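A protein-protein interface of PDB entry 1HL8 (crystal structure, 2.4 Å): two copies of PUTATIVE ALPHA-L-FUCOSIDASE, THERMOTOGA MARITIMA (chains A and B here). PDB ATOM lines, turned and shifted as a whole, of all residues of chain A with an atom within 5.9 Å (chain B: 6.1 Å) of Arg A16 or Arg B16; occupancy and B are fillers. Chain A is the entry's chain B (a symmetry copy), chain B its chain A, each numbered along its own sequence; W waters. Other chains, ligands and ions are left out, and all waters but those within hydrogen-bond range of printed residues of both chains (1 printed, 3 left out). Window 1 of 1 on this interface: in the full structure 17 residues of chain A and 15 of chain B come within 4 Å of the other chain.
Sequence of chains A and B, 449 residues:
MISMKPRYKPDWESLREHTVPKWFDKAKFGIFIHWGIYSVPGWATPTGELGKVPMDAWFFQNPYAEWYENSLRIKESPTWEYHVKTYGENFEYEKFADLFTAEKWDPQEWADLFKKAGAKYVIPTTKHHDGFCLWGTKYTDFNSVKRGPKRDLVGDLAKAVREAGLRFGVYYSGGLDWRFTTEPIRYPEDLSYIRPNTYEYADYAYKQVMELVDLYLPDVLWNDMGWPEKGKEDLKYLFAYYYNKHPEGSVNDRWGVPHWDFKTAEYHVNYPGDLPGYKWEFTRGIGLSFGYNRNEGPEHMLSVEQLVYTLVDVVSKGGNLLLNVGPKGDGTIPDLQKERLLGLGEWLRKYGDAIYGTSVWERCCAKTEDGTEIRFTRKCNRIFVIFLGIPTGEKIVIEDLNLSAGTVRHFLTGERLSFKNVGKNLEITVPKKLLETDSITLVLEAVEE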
ATOM      1  N   ASP A  11     -24.887  -4.477  -7.654  1.00  0.00           N
ATOM      2  CA  ASP A  11     -26.144  -5.213  -7.559  1.00  0.00           C
ATOM      3  C   ASP A  11     -26.116  -6.440  -8.445  1.00  0.00           C
ATOM      4  O   ASP A  11     -25.343  -6.521  -9.412  1.00  0.00           O
ATOM      5  CB  ASP A  11     -27.359  -4.336  -7.863  1.00  0.00           C
ATOM      6  CG  ASP A  11     -27.322  -3.747  -9.217  1.00  0.00           C
ATOM      7  OD1 ASP A  11     -26.819  -2.613  -9.332  1.00  0.00           O
ATOM      8  OD2 ASP A  11     -27.800  -4.317 -10.227  1.00  0.00           O
ATOM      9  N   TRP A  12     -26.953  -7.409  -8.109  1.00  0.00           N
ATOM     10  CA  TRP A  12     -26.845  -8.703  -8.764  1.00  0.00           C
ATOM     11  C   TRP A  12     -27.050  -8.589 -10.276  1.00  0.00           C
ATOM     12  O   TRP A  12     -26.311  -9.220 -11.033  1.00  0.00           O
ATOM     13  CB  TRP A  12     -27.770  -9.733  -8.125  1.00  0.00           C
ATOM     14  CG  TRP A  12     -27.604  -9.832  -6.630  1.00  0.00           C
ATOM     15  CD1 TRP A  12     -28.582  -9.659  -5.689  1.00  0.00           C
ATOM     16  CD2 TRP A  12     -26.399 -10.107  -5.906  1.00  0.00           C
ATOM     17  NE1 TRP A  12     -28.062  -9.826  -4.429  1.00  0.00           N
ATOM     18  CE2 TRP A  12     -26.725 -10.102  -4.530  1.00  0.00           C
ATOM     19  CE3 TRP A  12     -25.075 -10.385  -6.278  1.00  0.00           C
ATOM     20  CZ2 TRP A  12     -25.774 -10.346  -3.523  1.00  0.00           C
ATOM     21  CZ3 TRP A  12     -24.127 -10.623  -5.283  1.00  0.00           C
ATOM     22  CH2 TRP A  12     -24.480 -10.603  -3.926  1.00  0.00           C
ATOM     23  N   GLU A  13     -27.984  -7.741 -10.705  1.00  0.00           N
ATOM     24  CA  GLU A  13     -28.264  -7.557 -12.142  1.00  0.00           C
ATOM     25  C   GLU A  13     -27.041  -7.070 -12.932  1.00  0.00           C
ATOM     26  O   GLU A  13     -26.752  -7.572 -14.021  1.00  0.00           O
ATOM     27  CB  GLU A  13     -29.464  -6.609 -12.387  1.00  0.00           C
ATOM     28  CG  GLU A  13     -30.210  -6.956 -13.670  1.00  0.00           C
ATOM     29  CD  GLU A  13     -31.492  -6.153 -13.922  1.00  0.00           C
ATOM     30  OE1 GLU A  13     -31.875  -5.313 -13.067  1.00  0.00           O
ATOM     31  OE2 GLU A  13     -32.117  -6.375 -14.992  1.00  0.00           O
ATOM     32  N   SER A  14     -26.305  -6.120 -12.373  1.00  0.00           N
ATOM     33  CA  SER A  14     -25.109  -5.609 -13.041  1.00  0.00           C
ATOM     34  C   SER A  14     -23.939  -6.619 -13.012  1.00  0.00           C
ATOM     35  O   SER A  14     -23.228  -6.762 -13.996  1.00  0.00           O
ATOM     36  CB  SER A  14     -24.652  -4.290 -12.418  1.00  0.00           C
ATOM     37  OG  SER A  14     -23.345  -3.955 -12.855  1.00  0.00           O
ATOM     38  N   LEU A  15     -23.756  -7.315 -11.895  1.00  0.00           N
ATOM     39  CA  LEU A  15     -22.587  -8.178 -11.684  1.00  0.00           C
ATOM     40  C   LEU A  15     -22.610  -9.439 -12.540  1.00  0.00           C
ATOM     41  O   LEU A  15     -21.570 -10.063 -12.795  1.00  0.00           O
ATOM     42  CB  LEU A  15     -22.485  -8.590 -10.220  1.00  0.00           C
ATOM     43  CG  LEU A  15     -22.062  -7.490  -9.243  1.00  0.00           C
ATOM     44  CD1 LEU A  15     -22.348  -7.927  -7.821  1.00  0.00           C
ATOM     45  CD2 LEU A  15     -20.590  -7.139  -9.419  1.00  0.00           C
ATOM     46  N   ARG A  16     -23.802  -9.815 -12.983  1.00  0.00           N
ATOM     47  CA  ARG A  16     -23.952 -10.960 -13.856  1.00  0.00           C
ATOM     48  C   ARG A  16     -23.498 -10.628 -15.294  1.00  0.00           C
ATOM     49  O   ARG A  16     -23.388 -11.521 -16.114  1.00  0.00           O
ATOM     50  CB  ARG A  16     -25.390 -11.523 -13.792  1.00  0.00           C
ATOM     51  CG  ARG A  16     -26.330 -11.142 -14.922  1.00  0.00           C
ATOM     52  CD  ARG A  16     -27.564 -12.042 -15.043  1.00  0.00           C
ATOM     53  NE  ARG A  16     -27.223 -13.459 -15.162  1.00  0.00           N
ATOM     54  CZ  ARG A  16     -26.720 -14.041 -16.247  1.00  0.00           C
ATOM     55  NH1 ARG A  16     -26.475 -13.333 -17.349  1.00  0.00           N
ATOM     56  NH2 ARG A  16     -26.455 -15.348 -16.229  1.00  0.00           N
ATOM     57  N   GLU A  17     -23.191  -9.355 -15.561  1.00  0.00           N
ATOM     58  CA  GLU A  17     -22.386  -8.957 -16.726  1.00  0.00           C
ATOM     59  C   GLU A  17     -20.986  -9.563 -16.702  1.00  0.00           C
ATOM     60  O   GLU A  17     -20.395  -9.786 -17.753  1.00  0.00           O
ATOM     61  CB  GLU A  17     -22.232  -7.441 -16.818  1.00  0.00           C
ATOM     62  CG  GLU A  17     -23.511  -6.729 -17.177  1.00  0.00           C
ATOM     63  CD  GLU A  17     -23.439  -5.236 -16.961  1.00  0.00           C
ATOM     64  OE1 GLU A  17     -22.316  -4.701 -16.915  1.00  0.00           O
ATOM     65  OE2 GLU A  17     -24.515  -4.603 -16.847  1.00  0.00           O
ATOM     66  N   HIS A  18     -20.440  -9.791 -15.508  1.00  0.00           N
ATOM     67  CA  HIS A  18     -19.153 -10.458 -15.390  1.00  0.00           C
ATOM     68  C   HIS A  18     -19.292 -11.954 -15.683  1.00  0.00           C
ATOM     69  O   HIS A  18     -19.914 -12.688 -14.924  1.00  0.00           O
ATOM     70  CB  HIS A  18     -18.527 -10.235 -14.013  1.00  0.00           C
ATOM     71  CG  HIS A  18     -17.113 -10.703 -13.939  1.00  0.00           C
ATOM     72  ND1 HIS A  18     -16.099 -10.120 -14.661  1.00  0.00           N
ATOM     73  CD2 HIS A  18     -16.556 -11.747 -13.289  1.00  0.00           C
ATOM     74  CE1 HIS A  18     -14.971 -10.762 -14.432  1.00  0.00           C
ATOM     75  NE2 HIS A  18     -15.220 -11.755 -13.604  1.00  0.00           N
ATOM     76  N   THR A  19     -18.715 -12.395 -16.791  1.00  0.00           N
ATOM     77  CA  THR A  19     -18.700 -13.807 -17.151  1.00  0.00           C
ATOM     78  C   THR A  19     -17.334 -14.405 -16.837  1.00  0.00           C
ATOM     79  O   THR A  19     -16.340 -13.686 -16.748  1.00  0.00           O
ATOM     80  CB  THR A  19     -18.999 -13.983 -18.656  1.00  0.00           C
ATOM     81  OG1 THR A  19     -18.331 -12.966 -19.408  1.00  0.00           O
ATOM     82  CG2 THR A  19     -20.474 -13.733 -18.969  1.00  0.00           C
ATOM     83  N   VAL A  20     -17.287 -15.727 -16.708  1.00  0.00           N
ATOM     84  CA  VAL A  20     -16.032 -16.438 -16.499  1.00  0.00           C
ATOM     85  C   VAL A  20     -14.989 -15.996 -17.530  1.00  0.00           C
ATOM     86  O   VAL A  20     -15.262 -16.008 -18.729  1.00  0.00           O
ATOM     87  CB  VAL A  20     -16.214 -17.977 -16.545  1.00  0.00           C
ATOM     88  CG1 VAL A  20     -16.641 -18.470 -17.934  1.00  0.00           C
ATOM     89  CG2 VAL A  20     -14.936 -18.672 -16.073  1.00  0.00           C
ATOM     90  N   PRO A 258     -26.836 -14.755  -5.411  1.00  0.00           N
ATOM     91  CA  PRO A 258     -27.104 -14.938  -6.849  1.00  0.00           C
ATOM     92  C   PRO A 258     -26.012 -14.493  -7.834  1.00  0.00           C
ATOM     93  O   PRO A 258     -26.322 -13.952  -8.888  1.00  0.00           O
ATOM     94  CB  PRO A 258     -28.391 -14.120  -7.084  1.00  0.00           C
ATOM     95  CG  PRO A 258     -28.838 -13.633  -5.759  1.00  0.00           C
ATOM     96  CD  PRO A 258     -27.679 -13.693  -4.838  1.00  0.00           C
ATOM     97  N   HIS A 259     -24.751 -14.704  -7.518  1.00  0.00           N
ATOM     98  CA  HIS A 259     -23.703 -14.523  -8.509  1.00  0.00           C
ATOM     99  C   HIS A 259     -22.590 -15.531  -8.300  1.00  0.00           C
ATOM    100  O   HIS A 259     -22.288 -15.923  -7.177  1.00  0.00           O
ATOM    101  CB  HIS A 259     -23.141 -13.100  -8.491  1.00  0.00           C
ATOM    102  CG  HIS A 259     -22.079 -12.871  -9.521  1.00  0.00           C
ATOM    103  ND1 HIS A 259     -22.325 -12.964 -10.876  1.00  0.00           N
ATOM    104  CD2 HIS A 259     -20.757 -12.621  -9.395  1.00  0.00           C
ATOM    105  CE1 HIS A 259     -21.201 -12.758 -11.539  1.00  0.00           C
ATOM    106  NE2 HIS A 259     -20.235 -12.544 -10.665  1.00  0.00           N
ATOM    107  N   TRP A 260     -22.016 -15.965  -9.407  1.00  0.00           N
ATOM    108  CA  TRP A 260     -20.819 -16.786  -9.409  1.00  0.00           C
ATOM    109  C   TRP A 260     -20.298 -16.836 -10.841  1.00  0.00           C
ATOM    110  O   TRP A 260     -21.069 -16.686 -11.773  1.00  0.00           O
ATOM    111  CB  TRP A 260     -21.132 -18.208  -8.902  1.00  0.00           C
ATOM    112  CG  TRP A 260     -22.362 -18.842  -9.514  1.00  0.00           C
ATOM    113  CD1 TRP A 260     -23.623 -18.837  -8.995  1.00  0.00           C
ATOM    114  CD2 TRP A 260     -22.449 -19.564 -10.753  1.00  0.00           C
ATOM    115  NE1 TRP A 260     -24.486 -19.505  -9.829  1.00  0.00           N
ATOM    116  CE2 TRP A 260     -23.791 -19.966 -10.915  1.00  0.00           C
ATOM    117  CE3 TRP A 260     -21.525 -19.929 -11.737  1.00  0.00           C
ATOM    118  CZ2 TRP A 260     -24.231 -20.707 -12.019  1.00  0.00           C
ATOM    119  CZ3 TRP A 260     -21.966 -20.665 -12.847  1.00  0.00           C
ATOM    120  CH2 TRP A 260     -23.305 -21.036 -12.977  1.00  0.00           C
ATOM    121  N   ASP A 261     -19.004 -17.047 -11.021  1.00  0.00           N
ATOM    122  CA  ASP A 261     -18.426 -17.199 -12.359  1.00  0.00           C
ATOM    123  C   ASP A 261     -18.335 -18.651 -12.805  1.00  0.00           C
ATOM    124  O   ASP A 261     -18.441 -18.939 -13.992  1.00  0.00           O
ATOM    125  CB  ASP A 261     -17.043 -16.559 -12.413  1.00  0.00           C
ATOM    126  CG  ASP A 261     -17.094 -15.067 -12.186  1.00  0.00           C
ATOM    127  OD1 ASP A 261     -17.852 -14.387 -12.918  1.00  0.00           O
ATOM    128  OD2 ASP A 261     -16.415 -14.497 -11.303  1.00  0.00           O
ATOM    129  N   TYR A 278     -22.758 -23.865 -18.486  1.00  0.00           N
ATOM    130  CA  TYR A 278     -22.017 -23.024 -17.552  1.00  0.00           C
ATOM    131  C   TYR A 278     -20.660 -23.643 -17.244  1.00  0.00           C
ATOM    132  O   TYR A 278     -20.477 -24.852 -17.373  1.00  0.00           O
ATOM    133  CB  TYR A 278     -22.821 -22.840 -16.264  1.00  0.00           C
ATOM    134  CG  TYR A 278     -23.207 -24.119 -15.547  1.00  0.00           C
ATOM    135  CD1 TYR A 278     -22.366 -24.692 -14.603  1.00  0.00           C
ATOM    136  CD2 TYR A 278     -24.423 -24.738 -15.792  1.00  0.00           C
ATOM    137  CE1 TYR A 278     -22.726 -25.850 -13.930  1.00  0.00           C
ATOM    138  CE2 TYR A 278     -24.791 -25.896 -15.128  1.00  0.00           C
ATOM    139  CZ  TYR A 278     -23.940 -26.447 -14.199  1.00  0.00           C
ATOM    140  OH  TYR A 278     -24.289 -27.599 -13.529  1.00  0.00           O
ATOM    141  N   ASP B  11     -34.785 -20.156  -8.318  1.00  0.00           N
ATOM    142  CA  ASP B  11     -34.096 -19.166  -7.509  1.00  0.00           C
ATOM    143  C   ASP B  11     -33.002 -18.567  -8.364  1.00  0.00           C
ATOM    144  O   ASP B  11     -32.512 -19.208  -9.285  1.00  0.00           O
ATOM    145  CB  ASP B  11     -33.578 -19.743  -6.170  1.00  0.00           C
ATOM    146  CG  ASP B  11     -32.418 -20.677  -6.339  1.00  0.00           C
ATOM    147  OD1 ASP B  11     -32.669 -21.880  -6.564  1.00  0.00           O
ATOM    148  OD2 ASP B  11     -31.222 -20.307  -6.252  1.00  0.00           O
ATOM    149  N   TRP B  12     -32.647 -17.322  -8.087  1.00  0.00           N
ATOM    150  CA  TRP B  12     -31.784 -16.586  -9.001  1.00  0.00           C
ATOM    151  C   TRP B  12     -30.418 -17.244  -9.144  1.00  0.00           C
ATOM    152  O   TRP B  12     -29.930 -17.348 -10.238  1.00  0.00           O
ATOM    153  CB  TRP B  12     -31.633 -15.133  -8.586  1.00  0.00           C
ATOM    154  CG  TRP B  12     -32.918 -14.401  -8.370  1.00  0.00           C
ATOM    155  CD1 TRP B  12     -33.306 -13.796  -7.223  1.00  0.00           C
ATOM    156  CD2 TRP B  12     -33.977 -14.181  -9.320  1.00  0.00           C
ATOM    157  NE1 TRP B  12     -34.533 -13.214  -7.391  1.00  0.00           N
ATOM    158  CE2 TRP B  12     -34.970 -13.427  -8.666  1.00  0.00           C
ATOM    159  CE3 TRP B  12     -34.186 -14.541 -10.659  1.00  0.00           C
ATOM    160  CZ2 TRP B  12     -36.162 -13.030  -9.291  1.00  0.00           C
ATOM    161  CZ3 TRP B  12     -35.370 -14.147 -11.291  1.00  0.00           C
ATOM    162  CH2 TRP B  12     -36.342 -13.396 -10.601  1.00  0.00           C
ATOM    163  N   GLU B  13     -29.842 -17.713  -8.041  1.00  0.00           N
ATOM    164  CA  GLU B  13     -28.563 -18.437  -8.052  1.00  0.00           C
ATOM    165  C   GLU B  13     -28.581 -19.662  -8.976  1.00  0.00           C
ATOM    166  O   GLU B  13     -27.630 -19.898  -9.722  1.00  0.00           O
ATOM    167  CB  GLU B  13     -28.174 -18.873  -6.640  1.00  0.00           C
ATOM    168  CG  GLU B  13     -26.715 -19.286  -6.526  1.00  0.00           C
ATOM    169  CD  GLU B  13     -26.263 -19.602  -5.100  1.00  0.00           C
ATOM    170  OE1 GLU B  13     -27.088 -19.464  -4.154  1.00  0.00           O
ATOM    171  OE2 GLU B  13     -25.078 -19.991  -4.938  1.00  0.00           O
ATOM    172  N   SER B  14     -29.663 -20.430  -8.932  1.00  0.00           N
ATOM    173  CA  SER B  14     -29.803 -21.605  -9.797  1.00  0.00           C
ATOM    174  C   SER B  14     -30.044 -21.204 -11.254  1.00  0.00           C
ATOM    175  O   SER B  14     -29.589 -21.870 -12.168  1.00  0.00           O
ATOM    176  CB  SER B  14     -30.958 -22.498  -9.328  1.00  0.00           C
ATOM    177  OG  SER B  14     -31.596 -23.120 -10.435  1.00  0.00           O
ATOM    178  N   LEU B  15     -30.767 -20.115 -11.459  1.00  0.00           N
ATOM    179  CA  LEU B  15     -31.113 -19.666 -12.800  1.00  0.00           C
ATOM    180  C   LEU B  15     -29.924 -19.093 -13.575  1.00  0.00           C
ATOM    181  O   LEU B  15     -29.971 -19.054 -14.796  1.00  0.00           O
ATOM    182  CB  LEU B  15     -32.257 -18.646 -12.753  1.00  0.00           C
ATOM    183  CG  LEU B  15     -33.655 -19.194 -12.425  1.00  0.00           C
ATOM    184  CD1 LEU B  15     -34.637 -18.047 -12.150  1.00  0.00           C
ATOM    185  CD2 LEU B  15     -34.178 -20.066 -13.546  1.00  0.00           C
ATOM    186  N   ARG B  16     -28.854 -18.671 -12.895  1.00  0.00           N
ATOM    187  CA  ARG B  16     -27.645 -18.239 -13.617  1.00  0.00           C
ATOM    188  C   ARG B  16     -27.024 -19.422 -14.387  1.00  0.00           C
ATOM    189  O   ARG B  16     -26.255 -19.202 -15.320  1.00  0.00           O
ATOM    190  CB  ARG B  16     -26.587 -17.604 -12.687  1.00  0.00           C
ATOM    191  CG  ARG B  16     -25.156 -17.587 -13.294  1.00  0.00           C
ATOM    192  CD  ARG B  16     -24.251 -16.476 -12.842  1.00  0.00           C
ATOM    193  NE  ARG B  16     -24.162 -15.426 -13.861  1.00  0.00           N
ATOM    194  CZ  ARG B  16     -23.040 -14.931 -14.378  1.00  0.00           C
ATOM    195  NH1 ARG B  16     -23.118 -13.974 -15.286  1.00  0.00           N
ATOM    196  NH2 ARG B  16     -21.843 -15.364 -14.008  1.00  0.00           N
ATOM    197  N   GLU B  17     -27.344 -20.664 -14.006  1.00  0.00           N
ATOM    198  CA  GLU B  17     -26.875 -21.847 -14.769  1.00  0.00           C
ATOM    199  C   GLU B  17     -27.307 -21.798 -16.223  1.00  0.00           C
ATOM    200  O   GLU B  17     -26.625 -22.323 -17.080  1.00  0.00           O
ATOM    201  CB  GLU B  17     -27.370 -23.164 -14.163  1.00  0.00           C
ATOM    202  CG  GLU B  17     -26.824 -23.470 -12.785  1.00  0.00           C
ATOM    203  CD  GLU B  17     -27.514 -24.647 -12.123  1.00  0.00           C
ATOM    204  OE1 GLU B  17     -28.077 -25.502 -12.848  1.00  0.00           O
ATOM    205  OE2 GLU B  17     -27.492 -24.722 -10.873  1.00  0.00           O
ATOM    206  N   HIS B  18     -28.460 -21.198 -16.491  1.00  0.00           N
ATOM    207  CA  HIS B  18     -28.910 -21.000 -17.862  1.00  0.00           C
ATOM    208  C   HIS B  18     -28.162 -19.830 -18.491  1.00  0.00           C
ATOM    209  O   HIS B  18     -28.525 -18.674 -18.322  1.00  0.00           O
ATOM    210  CB  HIS B  18     -30.419 -20.750 -17.929  1.00  0.00           C
ATOM    211  CG  HIS B  18     -30.945 -20.635 -19.328  1.00  0.00           C
ATOM    212  ND1 HIS B  18     -30.965 -19.441 -20.015  1.00  0.00           N
ATOM    213  CD2 HIS B  18     -31.457 -21.564 -20.173  1.00  0.00           C
ATOM    214  CE1 HIS B  18     -31.456 -19.640 -21.224  1.00  0.00           C
ATOM    215  NE2 HIS B  18     -31.775 -20.918 -21.342  1.00  0.00           N
ATOM    216  N   THR B  19     -27.109 -20.145 -19.219  1.00  0.00           N
ATOM    217  CA  THR B  19     -26.420 -19.150 -20.033  1.00  0.00           C
ATOM    218  C   THR B  19     -27.140 -18.949 -21.358  1.00  0.00           C
ATOM    219  O   THR B  19     -28.037 -19.711 -21.726  1.00  0.00           O
ATOM    220  CB  THR B  19     -24.976 -19.576 -20.294  1.00  0.00           C
ATOM    221  OG1 THR B  19     -24.926 -20.987 -20.528  1.00  0.00           O
ATOM    222  CG2 THR B  19     -24.140 -19.375 -19.048  1.00  0.00           C
ATOM    223  N   PRO B 258     -32.598  -9.940 -10.998  1.00  0.00           N
ATOM    224  CA  PRO B 258     -31.196 -10.324 -11.189  1.00  0.00           C
ATOM    225  C   PRO B 258     -30.897 -11.116 -12.470  1.00  0.00           C
ATOM    226  O   PRO B 258     -29.836 -10.894 -13.056  1.00  0.00           O
ATOM    227  CB  PRO B 258     -30.901 -11.175  -9.955  1.00  0.00           C
ATOM    228  CG  PRO B 258     -31.865 -10.676  -8.920  1.00  0.00           C
ATOM    229  CD  PRO B 258     -33.119 -10.423  -9.703  1.00  0.00           C
ATOM    230  N   HIS B 259     -31.793 -11.984 -12.919  1.00  0.00           N
ATOM    231  CA  HIS B 259     -31.488 -12.850 -14.045  1.00  0.00           C
ATOM    232  C   HIS B 259     -31.868 -12.296 -15.419  1.00  0.00           C
ATOM    233  O   HIS B 259     -32.913 -11.685 -15.595  1.00  0.00           O
ATOM    234  CB  HIS B 259     -32.123 -14.218 -13.861  1.00  0.00           C
ATOM    235  CG  HIS B 259     -31.753 -15.178 -14.944  1.00  0.00           C
ATOM    236  ND1 HIS B 259     -30.483 -15.698 -15.070  1.00  0.00           N
ATOM    237  CD2 HIS B 259     -32.466 -15.665 -15.981  1.00  0.00           C
ATOM    238  CE1 HIS B 259     -30.433 -16.467 -16.142  1.00  0.00           C
ATOM    239  NE2 HIS B 259     -31.625 -16.465 -16.712  1.00  0.00           N
ATOM    240  N   TRP B 260     -30.972 -12.492 -16.379  1.00  0.00           N
ATOM    241  CA  TRP B 260     -31.218 -12.199 -17.792  1.00  0.00           C
ATOM    242  C   TRP B 260     -30.213 -12.988 -18.657  1.00  0.00           C
ATOM    243  O   TRP B 260     -29.148 -13.373 -18.178  1.00  0.00           O
ATOM    244  CB  TRP B 260     -31.115 -10.701 -18.076  1.00  0.00           C
ATOM    245  CG  TRP B 260     -29.885 -10.077 -17.545  1.00  0.00           C
ATOM    246  CD1 TRP B 260     -29.761  -9.402 -16.364  1.00  0.00           C
ATOM    247  CD2 TRP B 260     -28.584 -10.068 -18.151  1.00  0.00           C
ATOM    248  NE1 TRP B 260     -28.466  -8.977 -16.199  1.00  0.00           N
ATOM    249  CE2 TRP B 260     -27.721  -9.370 -17.281  1.00  0.00           C
ATOM    250  CE3 TRP B 260     -28.055 -10.585 -19.340  1.00  0.00           C
ATOM    251  CZ2 TRP B 260     -26.364  -9.174 -17.557  1.00  0.00           C
ATOM    252  CZ3 TRP B 260     -26.701 -10.384 -19.625  1.00  0.00           C
ATOM    253  CH2 TRP B 260     -25.870  -9.691 -18.729  1.00  0.00           C
ATOM    254  N   ASP B 261     -30.552 -13.221 -19.923  1.00  0.00           N
ATOM    255  CA  ASP B 261     -29.662 -13.930 -20.851  1.00  0.00           C
ATOM    256  C   ASP B 261     -28.880 -12.985 -21.768  1.00  0.00           C
ATOM    257  O   ASP B 261     -27.734 -13.273 -22.137  1.00  0.00           O
ATOM    258  CB  ASP B 261     -30.455 -14.922 -21.692  1.00  0.00           C
ATOM    259  CG  ASP B 261     -31.073 -16.013 -20.864  1.00  0.00           C
ATOM    260  OD1 ASP B 261     -30.339 -16.571 -20.004  1.00  0.00           O
ATOM    261  OD2 ASP B 261     -32.270 -16.384 -21.007  1.00  0.00           O
ATOM    262  N   PHE B 262     -29.509 -11.876 -22.146  1.00  0.00           N
ATOM    263  CA  PHE B 262     -28.844 -10.811 -22.888  1.00  0.00           C
ATOM    264  C   PHE B 262     -29.398  -9.444 -22.473  1.00  0.00           C
ATOM    265  O   PHE B 262     -30.540  -9.341 -22.017  1.00  0.00           O
ATOM    266  CB  PHE B 262     -28.987 -11.027 -24.400  1.00  0.00           C
ATOM    267  CG  PHE B 262     -30.414 -11.011 -24.895  1.00  0.00           C
ATOM    268  CD1 PHE B 262     -31.189 -12.156 -24.866  1.00  0.00           C
ATOM    269  CD2 PHE B 262     -30.979  -9.851 -25.394  1.00  0.00           C
ATOM    270  CE1 PHE B 262     -32.499 -12.134 -25.313  1.00  0.00           C
ATOM    271  CE2 PHE B 262     -32.281  -9.831 -25.850  1.00  0.00           C
ATOM    272  CZ  PHE B 262     -33.041 -10.968 -25.808  1.00  0.00           C
ATOM    273  N   TYR B 278     -20.388 -10.033 -22.061  1.00  0.00           N
ATOM    274  CA  TYR B 278     -21.737 -10.598 -22.004  1.00  0.00           C
ATOM    275  C   TYR B 278     -22.480 -10.323 -23.307  1.00  0.00           C
ATOM    276  O   TYR B 278     -22.151  -9.401 -24.046  1.00  0.00           O
ATOM    277  CB  TYR B 278     -22.518 -10.002 -20.822  1.00  0.00           C
ATOM    278  CG  TYR B 278     -22.639  -8.504 -20.904  1.00  0.00           C
ATOM    279  CD1 TYR B 278     -21.647  -7.669 -20.377  1.00  0.00           C
ATOM    280  CD2 TYR B 278     -23.715  -7.919 -21.547  1.00  0.00           C
ATOM    281  CE1 TYR B 278     -21.747  -6.297 -20.472  1.00  0.00           C
ATOM    282  CE2 TYR B 278     -23.824  -6.549 -21.653  1.00  0.00           C
ATOM    283  CZ  TYR B 278     -22.842  -5.745 -21.113  1.00  0.00           C
ATOM    284  OH  TYR B 278     -22.978  -4.388 -21.225  1.00  0.00           O
HETATM  285  O   HOH W   1     -22.609 -18.067  -5.067  1.00  0.00           O
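Trp A12 touches Pro B258, and with the chains exchanged Pro A258 touches Trp B12. Glu A13 touches Pro B258, and with the chains exchanged Pro A258 touches Glu B13. Arg A16 touches Trp B260, and with the chains exchanged Trp A260 touches Arg B16. Glu A17 touches Trp B260, and with the chains exchanged Trp A260 touches Glu B17. Positions printed for both chains: 11, 12, 13, 14, 15, 16, 17, 18, 19, 258, 259, 260, 261 and 278. Of the 17 pairs that touch across the chains among the printed residues, 15 have their exchanged pair printed and touching as well.
Glu A13 touches Pro B258 (CA to O, 3.8 Å). Arg A16 touches Pro B258 (CD to O, 3.2 Å). NE of Arg A16 touches ND1 of His B259, at 3.96 Å. N of Glu A17 touches CZ2 of Trp B260, 3.8 Å away. Glu A17 touches Tyr B278. Pro A258 touches Trp B12 (CB to CB, 3.7 Å). Glu B13 touches Pro A258. CE1 of His A259 touches NH2 of Arg B16 (3.6 Å). Glu B17 touches Trp A260 (N to CZ2, 3.7 Å). Glu B17 touches Tyr A278 (O to CD2, 3.5 Å).
Water W1 lies within hydrogen-bond range of the backbone carbonyl oxygen (O) of His A259 (3.0 Å) and the side-chain carboxylate (OE2) of Glu B13 (3.1 Å).
The backbone NH (N) of Glu A13 lies close to the side-chain carboxylate (OD2) of Asp A11 (3.5 Å). OD2 of Asp B11 lies close to N of Glu B13 (3.4 Å). The backbone carbonyl oxygen of Leu B15 sits close to a ring nitrogen (ND1) of His B259 (3.4 Å).
Printed residues of chain B within 4 Å of Arg A16: Arg B16, Pro B258, His B259 and Trp B260. Of the printed residues of chain A, Arg B16 touches Arg A16 (2.6 Å), His A18 (3.4 Å), His A259 (3.6 Å) and Trp A260 (2.7 Å). Of the printed residues of chain B, Trp A12 touches Pro B258. Of the printed residues of chain A, Pro B258 touches Trp A12 (3.9 Å), Glu A13 (3.8 Å) and Arg A16 (3.2 Å). Of the printed residues of chain A, Trp B12 touches Pro A258. The nearest printed residue of chain B that does not touch Arg A16 is His B18 (4.4 Å). The nearest printed residue of chain A that does not touch Arg B16 is Asp A261 (4.2 Å).
Of the 15 printed residues of chain A, 9 touch a printed residue of chain B. Hydrophobic or aromatic side chains of chain A that line the printed part of chain B: Trp A12, Pro A258, His A259, Trp A260 and Tyr A278. Hydrophobic or aromatic side chains of chain B that line the printed part of chain A: Trp B12, Pro B258, His B259, Trp B260 and Tyr B278. Among the printed residues, no Asp or Glu carboxylate lies within 4 Å of a Lys or Arg side-chain nitrogen of the other chain.
NH1 of Arg B16 lies within hydrogen-bond range of O of Arg A16. NE1 of Trp A260 lies within hydrogen-bond range of O of Glu B13 (3.2 Å). The indole nitrogen of Trp B260 is in hydrogen-bond range of the backbone carbonyl oxygen of Glu A13 (3.1 Å). NH2 of Arg B16 sits at hydrogen-bond distance from O of Trp A260, 2.7 Å away. The backbone carbonyl oxygen (O) of Trp B260 lies within hydrogen-bond range of the guanidinium group (NH1) of Arg A16. The guanidinium group of Arg B16 is in hydrogen-bond range of the backbone carbonyl oxygen of His A18 (3.4 Å).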
